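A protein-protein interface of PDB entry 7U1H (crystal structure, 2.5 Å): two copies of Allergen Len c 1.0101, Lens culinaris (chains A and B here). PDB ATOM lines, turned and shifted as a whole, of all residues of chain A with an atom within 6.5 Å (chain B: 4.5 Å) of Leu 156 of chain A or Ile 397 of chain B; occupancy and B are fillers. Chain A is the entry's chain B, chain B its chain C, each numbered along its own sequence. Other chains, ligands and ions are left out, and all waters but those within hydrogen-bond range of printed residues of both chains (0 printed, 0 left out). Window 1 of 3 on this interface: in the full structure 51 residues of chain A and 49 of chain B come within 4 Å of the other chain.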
ATOM      1  N   LEU A  79      -1.095 -35.571 -28.796  1.00  0.00           N
ATOM      2  CA  LEU A  79      -0.869 -34.433 -27.860  1.00  0.00           C
ATOM      3  C   LEU A  79      -1.242 -34.865 -26.446  1.00  0.00           C
ATOM      4  O   LEU A  79      -1.955 -35.854 -26.268  1.00  0.00           O
ATOM      5  CB  LEU A  79      -1.653 -33.200 -28.325  1.00  0.00           C
ATOM      6  CG  LEU A  79      -1.095 -32.539 -29.583  1.00  0.00           C
ATOM      7  CD1 LEU A  79      -1.977 -31.385 -30.023  1.00  0.00           C
ATOM      8  CD2 LEU A  79       0.324 -32.053 -29.364  1.00  0.00           C
ATOM      9  N   PRO A  80      -0.688 -34.177 -25.423  1.00  0.00           N
ATOM     10  CA  PRO A  80      -0.872 -34.537 -24.015  1.00  0.00           C
ATOM     11  C   PRO A  80      -2.329 -34.707 -23.573  1.00  0.00           C
ATOM     12  O   PRO A  80      -3.125 -33.820 -23.851  1.00  0.00           O
ATOM     13  CB  PRO A  80      -0.278 -33.349 -23.248  1.00  0.00           C
ATOM     14  CG  PRO A  80       0.741 -32.742 -24.192  1.00  0.00           C
ATOM     15  CD  PRO A  80       0.225 -33.038 -25.587  1.00  0.00           C
ATOM     16  N   GLN A  81      -2.612 -35.834 -22.906  1.00  0.00           N
ATOM     17  CA  GLN A  81      -3.955 -36.265 -22.449  1.00  0.00           C
ATOM     18  C   GLN A  81      -3.809 -37.316 -21.343  1.00  0.00           C
ATOM     19  O   GLN A  81      -2.704 -37.863 -21.129  1.00  0.00           O
ATOM     20  CB  GLN A  81      -4.746 -36.827 -23.629  1.00  0.00           C
ATOM     21  CG  GLN A  81      -4.153 -38.107 -24.210  1.00  0.00           C
ATOM     22  CD  GLN A  81      -5.010 -39.320 -23.913  1.00  0.00           C
ATOM     23  OE1 GLN A  81      -6.081 -39.480 -24.503  1.00  0.00           O
ATOM     24  NE2 GLN A  81      -4.567 -40.171 -22.986  1.00  0.00           N
ATOM     25  N   PHE A  82      -4.903 -37.577 -20.643  1.00  0.00           N
ATOM     26  CA  PHE A  82      -5.012 -38.658 -19.637  1.00  0.00           C
ATOM     27  C   PHE A  82      -6.454 -39.160 -19.673  1.00  0.00           C
ATOM     28  O   PHE A  82      -7.327 -38.429 -20.137  1.00  0.00           O
ATOM     29  CB  PHE A  82      -4.576 -38.153 -18.263  1.00  0.00           C
ATOM     30  CG  PHE A  82      -5.524 -37.148 -17.657  1.00  0.00           C
ATOM     31  CD1 PHE A  82      -5.267 -35.788 -17.746  1.00  0.00           C
ATOM     32  CD2 PHE A  82      -6.687 -37.562 -17.028  1.00  0.00           C
ATOM     33  CE1 PHE A  82      -6.141 -34.864 -17.204  1.00  0.00           C
ATOM     34  CE2 PHE A  82      -7.563 -36.634 -16.492  1.00  0.00           C
ATOM     35  CZ  PHE A  82      -7.284 -35.290 -16.579  1.00  0.00           C
ATOM     36  N   LEU A 101       4.375 -38.240 -17.582  1.00  0.00           N
ATOM     37  CA  LEU A 101       4.415 -37.144 -16.582  1.00  0.00           C
ATOM     38  C   LEU A 101       3.815 -37.630 -15.268  1.00  0.00           C
ATOM     39  O   LEU A 101       2.666 -38.148 -15.296  1.00  0.00           O
ATOM     40  CB  LEU A 101       3.613 -35.936 -17.082  1.00  0.00           C
ATOM     41  CG  LEU A 101       3.918 -35.408 -18.482  1.00  0.00           C
ATOM     42  CD1 LEU A 101       3.136 -34.120 -18.725  1.00  0.00           C
ATOM     43  CD2 LEU A 101       5.417 -35.184 -18.690  1.00  0.00           C
ATOM     44  N   SER A 103       3.532 -35.528 -11.263  1.00  0.00           N
ATOM     45  CA  SER A 103       3.225 -34.137 -10.837  1.00  0.00           C
ATOM     46  C   SER A 103       4.484 -33.257 -10.702  1.00  0.00           C
ATOM     47  O   SER A 103       4.338 -32.026 -10.824  1.00  0.00           O
ATOM     48  CB  SER A 103       2.450 -34.177  -9.557  1.00  0.00           C
ATOM     49  OG  SER A 103       3.209 -34.836  -8.561  1.00  0.00           O
ATOM     50  N   ILE A 124      -0.615 -38.183 -17.436  1.00  0.00           N
ATOM     51  CA  ILE A 124      -0.402 -37.410 -18.697  1.00  0.00           C
ATOM     52  C   ILE A 124       0.759 -38.037 -19.473  1.00  0.00           C
ATOM     53  O   ILE A 124       1.886 -38.136 -18.925  1.00  0.00           O
ATOM     54  CB  ILE A 124      -0.170 -35.907 -18.464  1.00  0.00           C
ATOM     55  CG1 ILE A 124      -1.198 -35.296 -17.502  1.00  0.00           C
ATOM     56  CG2 ILE A 124      -0.111 -35.189 -19.807  1.00  0.00           C
ATOM     57  CD1 ILE A 124      -1.969 -34.103 -18.015  1.00  0.00           C
ATOM     58  N   PHE A 154      -9.115 -36.690 -21.110  1.00  0.00           N
ATOM     59  CA  PHE A 154      -9.036 -35.227 -20.865  1.00  0.00           C
ATOM     60  C   PHE A 154      -7.865 -34.678 -21.686  1.00  0.00           C
ATOM     61  O   PHE A 154      -6.714 -35.089 -21.430  1.00  0.00           O
ATOM     62  CB  PHE A 154      -8.968 -34.942 -19.367  1.00  0.00           C
ATOM     63  CG  PHE A 154     -10.240 -35.214 -18.602  1.00  0.00           C
ATOM     64  CD1 PHE A 154     -10.653 -36.516 -18.341  1.00  0.00           C
ATOM     65  CD2 PHE A 154     -11.017 -34.177 -18.122  1.00  0.00           C
ATOM     66  CE1 PHE A 154     -11.812 -36.773 -17.622  1.00  0.00           C
ATOM     67  CE2 PHE A 154     -12.173 -34.436 -17.397  1.00  0.00           C
ATOM     68  CZ  PHE A 154     -12.572 -35.734 -17.151  1.00  0.00           C
ATOM     69  N   LEU A 155      -8.199 -33.876 -22.709  1.00  0.00           N
ATOM     70  CA  LEU A 155      -7.265 -33.256 -23.688  1.00  0.00           C
ATOM     71  C   LEU A 155      -6.772 -31.903 -23.146  1.00  0.00           C
ATOM     72  O   LEU A 155      -7.620 -31.003 -22.975  1.00  0.00           O
ATOM     73  CB  LEU A 155      -7.986 -33.066 -25.031  1.00  0.00           C
ATOM     74  CG  LEU A 155      -8.151 -34.310 -25.903  1.00  0.00           C
ATOM     75  CD1 LEU A 155      -6.831 -35.055 -26.025  1.00  0.00           C
ATOM     76  CD2 LEU A 155      -9.247 -35.230 -25.372  1.00  0.00           C
ATOM     77  N   LEU A 156      -5.469 -31.781 -22.860  1.00  0.00           N
ATOM     78  CA  LEU A 156      -4.790 -30.490 -22.537  1.00  0.00           C
ATOM     79  C   LEU A 156      -4.835 -29.594 -23.772  1.00  0.00           C
ATOM     80  O   LEU A 156      -4.906 -28.371 -23.598  1.00  0.00           O
ATOM     81  CB  LEU A 156      -3.319 -30.711 -22.141  1.00  0.00           C
ATOM     82  CG  LEU A 156      -3.013 -30.838 -20.648  1.00  0.00           C
ATOM     83  CD1 LEU A 156      -1.516 -30.985 -20.439  1.00  0.00           C
ATOM     84  CD2 LEU A 156      -3.548 -29.646 -19.845  1.00  0.00           C
ATOM     85  N   SER A 157      -4.796 -30.217 -24.953  1.00  0.00           N
ATOM     86  CA  SER A 157      -4.511 -29.572 -26.257  1.00  0.00           C
ATOM     87  C   SER A 157      -5.554 -28.485 -26.540  1.00  0.00           C
ATOM     88  O   SER A 157      -6.740 -28.864 -26.827  1.00  0.00           O
ATOM     89  CB  SER A 157      -4.449 -30.614 -27.354  1.00  0.00           C
ATOM     90  OG  SER A 157      -4.852 -31.896 -26.869  1.00  0.00           O
ATOM     91  N   GLY A 158      -5.130 -27.218 -26.410  1.00  0.00           N
ATOM     92  CA  GLY A 158      -5.751 -26.033 -27.026  1.00  0.00           C
ATOM     93  C   GLY A 158      -5.196 -25.854 -28.432  1.00  0.00           C
ATOM     94  O   GLY A 158      -4.007 -25.462 -28.570  1.00  0.00           O
ATOM     95  N   THR A 159      -5.998 -26.217 -29.439  1.00  0.00           N
ATOM     96  CA  THR A 159      -5.666 -26.150 -30.889  1.00  0.00           C
ATOM     97  C   THR A 159      -6.907 -25.651 -31.643  1.00  0.00           C
ATOM     98  O   THR A 159      -7.929 -25.396 -30.972  1.00  0.00           O
ATOM     99  CB  THR A 159      -5.146 -27.509 -31.392  1.00  0.00           C
ATOM    100  OG1 THR A 159      -5.962 -28.559 -30.861  1.00  0.00           O
ATOM    101  CG2 THR A 159      -3.697 -27.761 -31.028  1.00  0.00           C
ATOM    102  N   GLN A 162     -11.157 -28.939 -30.665  1.00  0.00           N
ATOM    103  CA  GLN A 162     -10.811 -29.658 -29.415  1.00  0.00           C
ATOM    104  C   GLN A 162     -10.349 -28.637 -28.369  1.00  0.00           C
ATOM    105  O   GLN A 162      -9.145 -28.459 -28.144  1.00  0.00           O
ATOM    106  CB  GLN A 162      -9.767 -30.725 -29.686  1.00  0.00           C
ATOM    107  N   PRO A 163     -11.299 -27.932 -27.700  1.00  0.00           N
ATOM    108  CA  PRO A 163     -10.955 -26.900 -26.715  1.00  0.00           C
ATOM    109  C   PRO A 163     -10.520 -27.488 -25.358  1.00  0.00           C
ATOM    110  O   PRO A 163     -11.303 -28.230 -24.786  1.00  0.00           O
ATOM    111  CB  PRO A 163     -12.275 -26.118 -26.583  1.00  0.00           C
ATOM    112  CG  PRO A 163     -13.355 -27.166 -26.815  1.00  0.00           C
ATOM    113  CD  PRO A 163     -12.758 -28.119 -27.834  1.00  0.00           C
ATOM    114  N   SER A 164      -9.319 -27.136 -24.875  1.00  0.00           N
ATOM    115  CA  SER A 164      -8.672 -27.652 -23.628  1.00  0.00           C
ATOM    116  C   SER A 164      -9.678 -27.809 -22.484  1.00  0.00           C
ATOM    117  O   SER A 164     -10.501 -26.894 -22.268  1.00  0.00           O
ATOM    118  CB  SER A 164      -7.546 -26.754 -23.179  1.00  0.00           C
ATOM    119  OG  SER A 164      -7.040 -27.169 -21.918  1.00  0.00           O
ATOM    120  N   PHE A 165      -9.584 -28.914 -21.742  1.00  0.00           N
ATOM    121  CA  PHE A 165     -10.461 -29.201 -20.571  1.00  0.00           C
ATOM    122  C   PHE A 165     -10.258 -28.104 -19.504  1.00  0.00           C
ATOM    123  O   PHE A 165     -11.162 -27.919 -18.665  1.00  0.00           O
ATOM    124  CB  PHE A 165     -10.238 -30.620 -20.028  1.00  0.00           C
ATOM    125  CG  PHE A 165      -8.948 -30.816 -19.268  1.00  0.00           C
ATOM    126  CD1 PHE A 165      -8.824 -30.393 -17.955  1.00  0.00           C
ATOM    127  CD2 PHE A 165      -7.852 -31.400 -19.871  1.00  0.00           C
ATOM    128  CE1 PHE A 165      -7.638 -30.552 -17.260  1.00  0.00           C
ATOM    129  CE2 PHE A 165      -6.670 -31.583 -19.171  1.00  0.00           C
ATOM    130  CZ  PHE A 165      -6.563 -31.153 -17.867  1.00  0.00           C
ATOM    131  N   LEU A 166      -9.146 -27.353 -19.557  1.00  0.00           N
ATOM    132  CA  LEU A 166      -8.926 -26.179 -18.659  1.00  0.00           C
ATOM    133  C   LEU A 166     -10.060 -25.159 -18.844  1.00  0.00           C
ATOM    134  O   LEU A 166     -10.347 -24.479 -17.858  1.00  0.00           O
ATOM    135  CB  LEU A 166      -7.552 -25.552 -18.912  1.00  0.00           C
ATOM    136  CG  LEU A 166      -6.362 -26.304 -18.313  1.00  0.00           C
ATOM    137  CD1 LEU A 166      -5.042 -25.660 -18.696  1.00  0.00           C
ATOM    138  CD2 LEU A 166      -6.474 -26.382 -16.814  1.00  0.00           C
ATOM    139  N   PHE A 178      -4.033 -19.417 -12.033  1.00  0.00           N
ATOM    140  CA  PHE A 178      -2.796 -19.065 -12.766  1.00  0.00           C
ATOM    141  C   PHE A 178      -2.363 -17.633 -12.371  1.00  0.00           C
ATOM    142  O   PHE A 178      -1.269 -17.234 -12.764  1.00  0.00           O
ATOM    143  CB  PHE A 178      -3.019 -19.302 -14.263  1.00  0.00           C
ATOM    144  CG  PHE A 178      -3.285 -20.736 -14.652  1.00  0.00           C
ATOM    145  CD1 PHE A 178      -2.245 -21.647 -14.750  1.00  0.00           C
ATOM    146  CD2 PHE A 178      -4.571 -21.179 -14.931  1.00  0.00           C
ATOM    147  CE1 PHE A 178      -2.481 -22.968 -15.097  1.00  0.00           C
ATOM    148  CE2 PHE A 178      -4.805 -22.501 -15.287  1.00  0.00           C
ATOM    149  CZ  PHE A 178      -3.758 -23.398 -15.357  1.00  0.00           C
ATOM    150  N   LEU A 189      -3.013 -20.540 -23.465  1.00  0.00           N
ATOM    151  CA  LEU A 189      -3.347 -21.954 -23.125  1.00  0.00           C
ATOM    152  C   LEU A 189      -4.605 -22.461 -23.843  1.00  0.00           C
ATOM    153  O   LEU A 189      -4.585 -23.636 -24.182  1.00  0.00           O
ATOM    154  CB  LEU A 189      -3.539 -22.111 -21.614  1.00  0.00           C
ATOM    155  CG  LEU A 189      -2.285 -21.983 -20.757  1.00  0.00           C
ATOM    156  CD1 LEU A 189      -2.588 -22.375 -19.319  1.00  0.00           C
ATOM    157  CD2 LEU A 189      -1.140 -22.820 -21.291  1.00  0.00           C
ATOM    158  N   LEU A 190      -5.677 -21.671 -24.002  1.00  0.00           N
ATOM    159  CA  LEU A 190      -7.016 -22.234 -24.352  1.00  0.00           C
ATOM    160  C   LEU A 190      -7.264 -22.199 -25.869  1.00  0.00           C
ATOM    161  O   LEU A 190      -7.068 -23.254 -26.488  1.00  0.00           O
ATOM    162  CB  LEU A 190      -8.105 -21.506 -23.562  1.00  0.00           C
ATOM    163  CG  LEU A 190      -7.907 -21.476 -22.045  1.00  0.00           C
ATOM    164  CD1 LEU A 190      -9.062 -20.764 -21.371  1.00  0.00           C
ATOM    165  CD2 LEU A 190      -7.756 -22.875 -21.473  1.00  0.00           C
ATOM    166  N   LEU B 389      -2.819 -28.446 -11.581  1.00  0.00           N
ATOM    167  CA  LEU B 389      -2.827 -27.877 -12.957  1.00  0.00           C
ATOM    168  C   LEU B 389      -2.349 -26.423 -12.957  1.00  0.00           C
ATOM    169  O   LEU B 389      -2.155 -25.895 -14.068  1.00  0.00           O
ATOM    170  CB  LEU B 389      -4.247 -27.954 -13.503  1.00  0.00           C
ATOM    171  CG  LEU B 389      -4.841 -29.359 -13.532  1.00  0.00           C
ATOM    172  CD1 LEU B 389      -6.340 -29.296 -13.764  1.00  0.00           C
ATOM    173  CD2 LEU B 389      -4.162 -30.215 -14.598  1.00  0.00           C
ATOM    174  N   ASN B 395       2.639 -29.256 -10.273  1.00  0.00           N
ATOM    175  CA  ASN B 395       2.062 -28.783 -11.552  1.00  0.00           C
ATOM    176  C   ASN B 395       2.573 -29.709 -12.668  1.00  0.00           C
ATOM    177  O   ASN B 395       3.758 -29.623 -13.086  1.00  0.00           O
ATOM    178  CB  ASN B 395       2.340 -27.307 -11.831  1.00  0.00           C
ATOM    179  CG  ASN B 395       1.532 -26.814 -13.017  1.00  0.00           C
ATOM    180  OD1 ASN B 395       1.102 -27.606 -13.861  1.00  0.00           O
ATOM    181  ND2 ASN B 395       1.291 -25.520 -13.085  1.00  0.00           N
ATOM    182  N   VAL B 396       1.692 -30.590 -13.119  1.00  0.00           N
ATOM    183  CA  VAL B 396       2.023 -31.619 -14.133  1.00  0.00           C
ATOM    184  C   VAL B 396       2.202 -30.901 -15.476  1.00  0.00           C
ATOM    185  O   VAL B 396       3.167 -31.222 -16.155  1.00  0.00           O
ATOM    186  CB  VAL B 396       0.957 -32.732 -14.135  1.00  0.00           C
ATOM    187  CG1 VAL B 396      -0.410 -32.235 -14.583  1.00  0.00           C
ATOM    188  CG2 VAL B 396       1.413 -33.934 -14.954  1.00  0.00           C
ATOM    189  N   ILE B 397       1.370 -29.909 -15.800  1.00  0.00           N
ATOM    190  CA  ILE B 397       1.507 -29.111 -17.059  1.00  0.00           C
ATOM    191  C   ILE B 397       2.959 -28.608 -17.217  1.00  0.00           C
ATOM    192  O   ILE B 397       3.457 -28.607 -18.346  1.00  0.00           O
ATOM    193  CB  ILE B 397       0.510 -27.936 -17.142  1.00  0.00           C
ATOM    194  CG1 ILE B 397      -0.944 -28.347 -16.858  1.00  0.00           C
ATOM    195  CG2 ILE B 397       0.653 -27.259 -18.496  1.00  0.00           C
ATOM    196  CD1 ILE B 397      -1.993 -27.249 -17.086  1.00  0.00           C
ATOM    197  N   SER B 398       3.623 -28.187 -16.145  1.00  0.00           N
ATOM    198  CA  SER B 398       5.006 -27.642 -16.178  1.00  0.00           C
ATOM    199  C   SER B 398       6.021 -28.719 -16.567  1.00  0.00           C
ATOM    200  O   SER B 398       7.160 -28.352 -16.917  1.00  0.00           O
ATOM    201  CB  SER B 398       5.373 -27.021 -14.855  1.00  0.00           C
ATOM    202  OG  SER B 398       4.577 -25.879 -14.650  1.00  0.00           O
ATOM    203  N   GLN B 399       5.629 -29.988 -16.468  1.00  0.00           N
ATOM    204  CA  GLN B 399       6.496 -31.155 -16.750  1.00  0.00           C
ATOM    205  C   GLN B 399       6.522 -31.445 -18.251  1.00  0.00           C
ATOM    206  O   GLN B 399       7.472 -32.097 -18.706  1.00  0.00           O
ATOM    207  CB  GLN B 399       5.985 -32.354 -15.961  1.00  0.00           C
ATOM    208  CG  GLN B 399       6.071 -32.166 -14.457  1.00  0.00           C
ATOM    209  CD  GLN B 399       7.506 -31.929 -14.079  1.00  0.00           C
ATOM    210  OE1 GLN B 399       8.428 -32.432 -14.734  1.00  0.00           O
ATOM    211  NE2 GLN B 399       7.690 -31.137 -13.036  1.00  0.00           N
ATOM    212  N   ILE B 400       5.510 -30.997 -18.993  1.00  0.00           N
ATOM    213  CA  ILE B 400       5.504 -31.080 -20.485  1.00  0.00           C
ATOM    214  C   ILE B 400       6.835 -30.493 -20.973  1.00  0.00           C
ATOM    215  O   ILE B 400       7.104 -29.330 -20.611  1.00  0.00           O
ATOM    216  CB  ILE B 400       4.315 -30.307 -21.087  1.00  0.00           C
ATOM    217  CG1 ILE B 400       2.963 -30.766 -20.540  1.00  0.00           C
ATOM    218  CG2 ILE B 400       4.351 -30.403 -22.596  1.00  0.00           C
ATOM    219  CD1 ILE B 400       1.831 -29.817 -20.823  1.00  0.00           C
ATOM    220  N   LYS B 405       5.127 -28.018 -25.310  1.00  0.00           N
ATOM    221  CA  LYS B 405       4.411 -26.771 -24.916  1.00  0.00           C
ATOM    222  C   LYS B 405       4.110 -25.929 -26.166  1.00  0.00           C
ATOM    223  O   LYS B 405       2.953 -25.548 -26.287  1.00  0.00           O
ATOM    224  CB  LYS B 405       5.192 -26.000 -23.864  1.00  0.00           C
ATOM    225  CG  LYS B 405       5.048 -26.564 -22.467  1.00  0.00           C
ATOM    226  CD  LYS B 405       6.090 -26.024 -21.495  1.00  0.00           C
ATOM    227  CE  LYS B 405       5.686 -26.222 -20.055  1.00  0.00           C
ATOM    228  NZ  LYS B 405       6.855 -26.143 -19.155  1.00  0.00           N
ATOM    229  N   PHE B 409      -0.108 -25.999 -27.080  1.00  0.00           N
ATOM    230  CA  PHE B 409      -0.714 -24.728 -26.622  1.00  0.00           C
ATOM    231  C   PHE B 409      -0.625 -23.685 -27.728  1.00  0.00           C
ATOM    232  O   PHE B 409       0.376 -23.574 -28.438  1.00  0.00           O
ATOM    233  CB  PHE B 409      -0.069 -24.301 -25.300  1.00  0.00           C
ATOM    234  CG  PHE B 409      -0.425 -25.188 -24.132  1.00  0.00           C
ATOM    235  CD1 PHE B 409       0.559 -25.829 -23.399  1.00  0.00           C
ATOM    236  CD2 PHE B 409      -1.752 -25.396 -23.777  1.00  0.00           C
ATOM    237  CE1 PHE B 409       0.220 -26.666 -22.349  1.00  0.00           C
ATOM    238  CE2 PHE B 409      -2.083 -26.246 -22.739  1.00  0.00           C
ATOM    239  CZ  PHE B 409      -1.096 -26.889 -22.034  1.00  0.00           C
ATOM    240  N   LEU B 420       2.683 -20.084 -16.561  1.00  0.00           N
ATOM    241  CA  LEU B 420       2.818 -21.102 -15.477  1.00  0.00           C
ATOM    242  C   LEU B 420       3.591 -20.595 -14.250  1.00  0.00           C
ATOM    243  O   LEU B 420       3.353 -21.181 -13.198  1.00  0.00           O
ATOM    244  CB  LEU B 420       3.499 -22.349 -16.044  1.00  0.00           C
ATOM    245  CG  LEU B 420       2.683 -23.088 -17.107  1.00  0.00           C
ATOM    246  CD1 LEU B 420       3.325 -24.425 -17.478  1.00  0.00           C
ATOM    247  CD2 LEU B 420       1.232 -23.272 -16.649  1.00  0.00           C
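Printed residues of chain B that touch a printed residue of chain A: Leu 389, Asn 395, Val 396, Ile 397, Gln 399, Ile 400 and Phe 409.
Hydrophobic or aromatic side chains of chain A that line the printed part of chain B: Leu 101, Ile 124, Leu 156, Phe 165, Leu 166, Phe 178 and Leu 189.
Among the printed residues, no Asp or Glu carboxylate lies within 4 Å of a Lys or Arg side-chain nitrogen of the other chain.
No position is printed for both chains.
Of the 14 pairs that touch across the chains among the printed residues, none has its exchanged pair printed and touching as well.
Leu 79 of chain A touches none of the printed residues of chain B.
Of the printed residues of chain B, Ser 103 of chain A touches Asn 395 and Val 396.
Printed residues of chain B within 4 Å of Ile 124 of chain A: Val 396 (3.9 Å).
Leu 156 of chain A touches just these residues of chain B: Ile 397, Ile 400 and Phe 409.
Of the printed residues of chain B, Phe 165 of chain A touches Leu 389 (3.9 Å).
Printed residues of chain B within 4 Å of Leu 189 of chain A: Phe 409.
Of the printed residues of chain A, Gln 399 of chain B touches Leu 101.
The nearest printed residue of chain B that does not touch Leu 156 of chain A is Leu 389 of chain B (5.3 Å).
The nearest printed residue of chain A that does not touch Val 396 of chain B is Leu 156 of chain A (6.1 Å).
The backbone carbonyl oxygen (O) of Ser 103 of chain A sits at hydrogen-bond distance from the backbone NH (N) of Asn 395 of chain B (3.3 Å).
CD2 of Leu 101 of chain A touches O of Gln 399 of chain B, 3.7 Å away.
Leu 101 of chain A touches Ile 400 of chain B.
Ser 103 of chain A touches Val 396 of chain B (O to N, 3.8 Å).
Ile 124 of chain A touches Val 396 of chain B (CG1 to CG2, 3.9 Å).
Leu 156 of chain A touches Ile 397 of chain B.
Leu 156 of chain A touches Ile 400 of chain B.
Phe 409 of chain B touches Gly 158 of chain A.
CD1 of Leu 166 of chain A touches CD1 of Ile 397 of chain B, 3.8 Å away.
Phe 178 of chain A touches Leu 389 of chain B (CE1 to O, 3.1 Å).
Leu 189 of chain A touches Phe 409 of chain B.
The backbone NH of Leu 156 of chain A sits at hydrogen-bond distance from the backbone carbonyl oxygen of Pro 80 of chain A, 3.3 Å away.
N of Leu 101 of chain A sits at hydrogen-bond distance from O of Ile 124 of chain A, 2.8 Å away.
O of Leu 155 of chain A is in hydrogen-bond range of N of Phe 165 of chain A (3.1 Å).
The backbone carbonyl oxygen of Leu 156 of chain A sits at hydrogen-bond distance from the side-chain hydroxyl of Ser 164 of chain A (3.0 Å).
The backbone NH (N) of Leu 166 of chain A lies close to the side-chain hydroxyl (OG) of Ser 164 of chain A, 3.2 Å away.
N of Ile 397 of chain B is in hydrogen-bond range of OD1 of Asn 395 of chain B, 3.0 Å away.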
